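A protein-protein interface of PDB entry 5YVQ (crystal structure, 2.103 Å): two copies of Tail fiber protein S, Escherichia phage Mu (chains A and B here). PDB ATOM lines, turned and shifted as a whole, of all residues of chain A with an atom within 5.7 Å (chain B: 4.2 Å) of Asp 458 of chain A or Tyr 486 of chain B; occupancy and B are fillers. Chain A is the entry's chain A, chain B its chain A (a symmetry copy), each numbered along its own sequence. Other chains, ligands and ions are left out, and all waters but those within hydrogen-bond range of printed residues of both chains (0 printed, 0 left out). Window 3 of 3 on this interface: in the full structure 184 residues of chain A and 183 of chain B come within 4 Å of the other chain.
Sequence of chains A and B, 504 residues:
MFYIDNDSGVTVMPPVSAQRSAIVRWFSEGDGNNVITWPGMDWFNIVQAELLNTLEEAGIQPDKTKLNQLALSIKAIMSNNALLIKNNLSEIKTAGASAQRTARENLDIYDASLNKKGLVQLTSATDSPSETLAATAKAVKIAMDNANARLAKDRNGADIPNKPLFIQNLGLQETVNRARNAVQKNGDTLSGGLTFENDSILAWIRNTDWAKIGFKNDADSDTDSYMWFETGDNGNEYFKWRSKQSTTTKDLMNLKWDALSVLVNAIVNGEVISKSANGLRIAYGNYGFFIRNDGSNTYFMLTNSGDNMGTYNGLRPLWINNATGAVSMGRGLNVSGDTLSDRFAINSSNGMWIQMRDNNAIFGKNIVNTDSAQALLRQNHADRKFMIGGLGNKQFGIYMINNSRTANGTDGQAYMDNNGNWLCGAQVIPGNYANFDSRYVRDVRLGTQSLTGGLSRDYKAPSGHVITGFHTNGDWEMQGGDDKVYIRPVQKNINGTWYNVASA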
ATOM      1  N   SER A 456     -18.826  10.707  32.073  1.00  0.00           N
ATOM      2  CA  SER A 456     -17.454  10.250  31.917  1.00  0.00           C
ATOM      3  C   SER A 456     -16.548  11.349  31.369  1.00  0.00           C
ATOM      4  O   SER A 456     -16.986  12.433  30.971  1.00  0.00           O
ATOM      5  CB  SER A 456     -17.407   9.032  30.996  1.00  0.00           C
ATOM      6  OG  SER A 456     -18.163   9.254  29.819  1.00  0.00           O
ATOM      7  N   ARG A 457     -15.251  11.037  31.354  1.00  0.00           N
ATOM      8  CA  ARG A 457     -14.234  11.930  30.820  1.00  0.00           C
ATOM      9  C   ARG A 457     -14.299  12.054  29.303  1.00  0.00           C
ATOM     10  O   ARG A 457     -13.587  12.891  28.742  1.00  0.00           O
ATOM     11  CB  ARG A 457     -12.848  11.445  31.251  1.00  0.00           C
ATOM     12  CG  ARG A 457     -12.640  11.447  32.761  1.00  0.00           C
ATOM     13  CD  ARG A 457     -11.176  11.637  33.133  1.00  0.00           C
ATOM     14  NE  ARG A 457     -11.025  12.321  34.417  1.00  0.00           N
ATOM     15  CZ  ARG A 457      -9.905  12.910  34.824  1.00  0.00           C
ATOM     16  NH1 ARG A 457      -8.828  12.900  34.051  1.00  0.00           N
ATOM     17  NH2 ARG A 457      -9.863  13.511  36.005  1.00  0.00           N
ATOM     18  N   ASP A 458     -15.126  11.251  28.636  1.00  0.00           N
ATOM     19  CA  ASP A 458     -15.319  11.316  27.192  1.00  0.00           C
ATOM     20  C   ASP A 458     -16.815  11.346  26.907  1.00  0.00           C
ATOM     21  O   ASP A 458     -17.558  10.499  27.414  1.00  0.00           O
ATOM     22  CB  ASP A 458     -14.654  10.123  26.491  1.00  0.00           C
ATOM     23  CG  ASP A 458     -15.062   9.991  25.030  1.00  0.00           C
ATOM     24  OD1 ASP A 458     -16.157   9.453  24.752  1.00  0.00           O
ATOM     25  OD2 ASP A 458     -14.282  10.421  24.154  1.00  0.00           O
ATOM     26  N   TYR A 459     -17.254  12.314  26.101  1.00  0.00           N
ATOM     27  CA  TYR A 459     -18.672  12.457  25.797  1.00  0.00           C
ATOM     28  C   TYR A 459     -18.855  12.971  24.373  1.00  0.00           C
ATOM     29  O   TYR A 459     -18.087  13.815  23.908  1.00  0.00           O
ATOM     30  CB  TYR A 459     -19.367  13.405  26.783  1.00  0.00           C
ATOM     31  CG  TYR A 459     -20.787  13.699  26.377  1.00  0.00           C
ATOM     32  CD1 TYR A 459     -21.730  12.680  26.311  1.00  0.00           C
ATOM     33  CD2 TYR A 459     -21.175  14.979  26.013  1.00  0.00           C
ATOM     34  CE1 TYR A 459     -23.027  12.931  25.918  1.00  0.00           C
ATOM     35  CE2 TYR A 459     -22.474  15.244  25.609  1.00  0.00           C
ATOM     36  CZ  TYR A 459     -23.397  14.217  25.562  1.00  0.00           C
ATOM     37  OH  TYR A 459     -24.692  14.474  25.160  1.00  0.00           O
ATOM     38  N   LYS A 460     -19.883  12.458  23.693  1.00  0.00           N
ATOM     39  CA  LYS A 460     -20.271  12.916  22.361  1.00  0.00           C
ATOM     40  C   LYS A 460     -21.756  13.255  22.352  1.00  0.00           C
ATOM     41  O   LYS A 460     -22.580  12.451  22.802  1.00  0.00           O
ATOM     42  CB  LYS A 460     -19.982  11.855  21.289  1.00  0.00           C
ATOM     43  CG  LYS A 460     -18.602  11.234  21.355  1.00  0.00           C
ATOM     44  CD  LYS A 460     -18.396  10.239  20.222  1.00  0.00           C
ATOM     45  CE  LYS A 460     -17.172   9.371  20.450  1.00  0.00           C
ATOM     46  NZ  LYS A 460     -16.808   8.595  19.236  1.00  0.00           N
ATOM     47  N   GLN B 449     -17.766  14.418  12.817  1.00  0.00           N
ATOM     48  CA  GLN B 449     -17.145  14.812  14.074  1.00  0.00           C
ATOM     49  C   GLN B 449     -15.630  14.619  14.018  1.00  0.00           C
ATOM     50  O   GLN B 449     -15.136  13.593  13.541  1.00  0.00           O
ATOM     51  CB  GLN B 449     -17.750  13.985  15.206  1.00  0.00           C
ATOM     52  CG  GLN B 449     -17.472  14.491  16.601  1.00  0.00           C
ATOM     53  CD  GLN B 449     -18.259  13.723  17.645  1.00  0.00           C
ATOM     54  OE1 GLN B 449     -18.911  14.318  18.501  1.00  0.00           O
ATOM     55  NE2 GLN B 449     -18.196  12.396  17.584  1.00  0.00           N
ATOM     56  N   SER B 450     -14.889  15.614  14.497  1.00  0.00           N
ATOM     57  CA  SER B 450     -13.441  15.525  14.620  1.00  0.00           C
ATOM     58  C   SER B 450     -13.033  15.916  16.036  1.00  0.00           C
ATOM     59  O   SER B 450     -13.824  16.479  16.798  1.00  0.00           O
ATOM     60  CB  SER B 450     -12.720  16.418  13.596  1.00  0.00           C
ATOM     61  OG  SER B 450     -12.584  17.748  14.068  1.00  0.00           O
ATOM     62  N   LEU B 451     -11.787  15.609  16.387  1.00  0.00           N
ATOM     63  CA  LEU B 451     -11.239  15.976  17.686  1.00  0.00           C
ATOM     64  C   LEU B 451     -10.050  16.904  17.536  1.00  0.00           C
ATOM     65  O   LEU B 451      -9.167  16.673  16.706  1.00  0.00           O
ATOM     66  CB  LEU B 451     -10.806  14.762  18.498  1.00  0.00           C
ATOM     67  CG  LEU B 451     -11.927  14.447  19.475  1.00  0.00           C
ATOM     68  CD1 LEU B 451     -12.950  13.685  18.683  1.00  0.00           C
ATOM     69  CD2 LEU B 451     -11.475  13.687  20.722  1.00  0.00           C
ATOM     70  N   ILE B 467     -19.059  23.042  18.990  1.00  0.00           N
ATOM     71  CA  ILE B 467     -18.592  22.017  19.919  1.00  0.00           C
ATOM     72  C   ILE B 467     -19.690  20.985  20.139  1.00  0.00           C
ATOM     73  O   ILE B 467     -20.835  21.326  20.465  1.00  0.00           O
ATOM     74  CB  ILE B 467     -18.146  22.638  21.250  1.00  0.00           C
ATOM     75  CG1 ILE B 467     -16.730  23.181  21.112  1.00  0.00           C
ATOM     76  CG2 ILE B 467     -18.181  21.602  22.373  1.00  0.00           C
ATOM     77  CD1 ILE B 467     -16.524  24.432  21.851  1.00  0.00           C
ATOM     78  N   THR B 468     -19.330  19.709  19.985  1.00  0.00           N
ATOM     79  CA  THR B 468     -20.269  18.606  20.116  1.00  0.00           C
ATOM     80  C   THR B 468     -19.831  17.551  21.132  1.00  0.00           C
ATOM     81  O   THR B 468     -20.486  16.507  21.235  1.00  0.00           O
ATOM     82  CB  THR B 468     -20.487  17.940  18.751  1.00  0.00           C
ATOM     83  OG1 THR B 468     -19.212  17.697  18.142  1.00  0.00           O
ATOM     84  CG2 THR B 468     -21.331  18.838  17.826  1.00  0.00           C
ATOM     85  N   GLY B 469     -18.758  17.772  21.882  1.00  0.00           N
ATOM     86  CA  GLY B 469     -18.396  16.803  22.903  1.00  0.00           C
ATOM     87  C   GLY B 469     -17.119  17.174  23.626  1.00  0.00           C
ATOM     88  O   GLY B 469     -16.566  18.259  23.445  1.00  0.00           O
ATOM     89  N   PHE B 470     -16.658  16.243  24.464  1.00  0.00           N
ATOM     90  CA  PHE B 470     -15.463  16.446  25.274  1.00  0.00           C
ATOM     91  C   PHE B 470     -14.728  15.127  25.450  1.00  0.00           C
ATOM     92  O   PHE B 470     -15.315  14.047  25.348  1.00  0.00           O
ATOM     93  CB  PHE B 470     -15.790  17.024  26.656  1.00  0.00           C
ATOM     94  CG  PHE B 470     -16.740  18.181  26.625  1.00  0.00           C
ATOM     95  CD1 PHE B 470     -18.086  17.992  26.884  1.00  0.00           C
ATOM     96  CD2 PHE B 470     -16.287  19.460  26.342  1.00  0.00           C
ATOM     97  CE1 PHE B 470     -18.968  19.058  26.856  1.00  0.00           C
ATOM     98  CE2 PHE B 470     -17.164  20.527  26.312  1.00  0.00           C
ATOM     99  CZ  PHE B 470     -18.504  20.327  26.570  1.00  0.00           C
ATOM    100  N   HIS B 471     -13.429  15.233  25.721  1.00  0.00           N
ATOM    101  CA  HIS B 471     -12.617  14.077  26.095  1.00  0.00           C
ATOM    102  C   HIS B 471     -11.525  14.562  27.038  1.00  0.00           C
ATOM    103  O   HIS B 471     -10.611  15.274  26.614  1.00  0.00           O
ATOM    104  CB  HIS B 471     -12.019  13.386  24.872  1.00  0.00           C
ATOM    105  CG  HIS B 471     -11.149  12.215  25.211  1.00  0.00           C
ATOM    106  ND1 HIS B 471     -11.644  10.938  25.365  1.00  0.00           N
ATOM    107  CD2 HIS B 471      -9.815  12.130  25.435  1.00  0.00           C
ATOM    108  CE1 HIS B 471     -10.653  10.116  25.664  1.00  0.00           C
ATOM    109  NE2 HIS B 471      -9.534  10.814  25.713  1.00  0.00           N
ATOM    110  N   VAL B 485     -11.675  18.224  22.911  1.00  0.00           N
ATOM    111  CA  VAL B 485     -13.048  18.640  22.647  1.00  0.00           C
ATOM    112  C   VAL B 485     -13.456  18.144  21.265  1.00  0.00           C
ATOM    113  O   VAL B 485     -12.663  18.178  20.318  1.00  0.00           O
ATOM    114  CB  VAL B 485     -13.213  20.174  22.777  1.00  0.00           C
ATOM    115  CG1 VAL B 485     -12.332  20.915  21.790  1.00  0.00           C
ATOM    116  CG2 VAL B 485     -14.655  20.578  22.603  1.00  0.00           C
ATOM    117  N   TYR B 486     -14.687  17.646  21.167  1.00  0.00           N
ATOM    118  CA  TYR B 486     -15.270  17.220  19.902  1.00  0.00           C
ATOM    119  C   TYR B 486     -15.881  18.423  19.195  1.00  0.00           C
ATOM    120  O   TYR B 486     -16.419  19.324  19.848  1.00  0.00           O
ATOM    121  CB  TYR B 486     -16.352  16.163  20.133  1.00  0.00           C
ATOM    122  CG  TYR B 486     -15.856  14.822  20.628  1.00  0.00           C
ATOM    123  CD1 TYR B 486     -16.112  13.668  19.907  1.00  0.00           C
ATOM    124  CD2 TYR B 486     -15.151  14.705  21.823  1.00  0.00           C
ATOM    125  CE1 TYR B 486     -15.663  12.441  20.337  1.00  0.00           C
ATOM    126  CE2 TYR B 486     -14.703  13.477  22.266  1.00  0.00           C
ATOM    127  CZ  TYR B 486     -14.963  12.349  21.518  1.00  0.00           C
ATOM    128  OH  TYR B 486     -14.522  11.118  21.946  1.00  0.00           O
ATOM    129  N   ILE B 487     -15.805  18.434  17.857  1.00  0.00           N
ATOM    130  CA  ILE B 487     -16.423  19.483  17.054  1.00  0.00           C
ATOM    131  C   ILE B 487     -17.024  18.876  15.790  1.00  0.00           C
ATOM    132  O   ILE B 487     -16.588  17.823  15.314  1.00  0.00           O
ATOM    133  CB  ILE B 487     -15.437  20.615  16.666  1.00  0.00           C
ATOM    134  CG1 ILE B 487     -14.246  20.057  15.885  1.00  0.00           C
ATOM    135  CG2 ILE B 487     -14.987  21.415  17.889  1.00  0.00           C
ATOM    136  CD1 ILE B 487     -13.418  21.130  15.196  1.00  0.00           C
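O of Arg 457 of chain A touches O of Phe 470 of chain B, at 3.98 Å.
His 471 of chain B touches Arg 457 of chain A.
Asp 458 of chain A touches Phe 470 of chain B (CA to O, 3.3 Å).
CA of Gly 469 of chain B touches O of Tyr 459 of chain A (3.2 Å).
CD2 of Tyr 486 of chain B touches O of Tyr 459 of chain A (3.7 Å).
Lys 460 of chain A touches Gln 449 of chain B.
O of Thr 468 of chain B touches C of Lys 460 of chain A, 3.7 Å away.
Tyr 486 of chain B touches Lys 460 of chain A (CE1 to CG, 3.3 Å).
OD2 of Asp 458 of chain A sits at hydrogen-bond distance from ND1 of His 471 of chain B, at 2.9 Å.
The backbone NH of Tyr 459 of chain A lies within hydrogen-bond range of the backbone carbonyl oxygen of Phe 470 of chain B (2.7 Å).
The side-chain carboxylate (OD2) of Asp 458 of chain A lies close to the side-chain hydroxyl (OH) of Tyr 486 of chain B, at 2.3 Å.
No position is printed for both chains.
Ser 456 of chain A touches none of the printed residues of chain B.
Of the printed residues of chain B, Asp 458 of chain A touches Phe 470, His 471 and Tyr 486.
Of the printed residues of chain B, Tyr 459 of chain A touches Gly 469 (3.2 Å), Phe 470 (2.7 Å) and Tyr 486 (3.7 Å).
Ile 467 of chain B touches none of the printed residues of chain A.
Printed residues of chain A within 4 Å of Phe 470 of chain B: Arg 457 (3.98 Å), Asp 458 (3.3 Å) and Tyr 459 (2.7 Å).
Of chain A, only Asp 458 (2.3 Å), Tyr 459 (3.7 Å) and Lys 460 (3.3 Å) come within 4 Å of Tyr 486 of chain B.
The nearest printed residue of chain B that does not touch Asp 458 of chain A is Leu 451 of chain B (5.5 Å).
The nearest printed residue of chain A that does not touch Tyr 486 of chain B is Arg 457 of chain A (6.6 Å).
The nearest printed residue of chain B that does not touch Lys 460 of chain A is Gly 469 of chain B (4.3 Å).
The side-chain hydroxyl of Ser 456 of chain A lies within hydrogen-bond range of the backbone carbonyl oxygen of Asp 458 of chain A (2.8 Å).
OG1 of Thr 468 of chain B is in hydrogen-bond range of OE1 of Gln 449 of chain B (3.4 Å).
O of Tyr 486 of chain B lies within hydrogen-bond range of N of Thr 468 of chain B.
The backbone NH of Ile 487 of chain B lies close to the side-chain hydroxyl of Thr 468 of chain B.
The backbone carbonyl oxygen (O) of Gly 469 of chain B lies within hydrogen-bond range of the backbone NH (N) of Tyr 486 of chain B (3.0 Å).
Of the 5 printed residues of chain A, 4 touch a printed residue of chain B.
Printed residues of chain A that touch a printed residue of chain B: Arg 457, Asp 458, Tyr 459 and Lys 460.
Along chain A the printed residues that touch a printed residue of chain B span positions 457 to 460.
Among the printed residues, 11 pairs touch across the chains.
Among the printed residues, no Asp or Glu carboxylate lies within 4 Å of a Lys or Arg side-chain nitrogen of the other chain.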
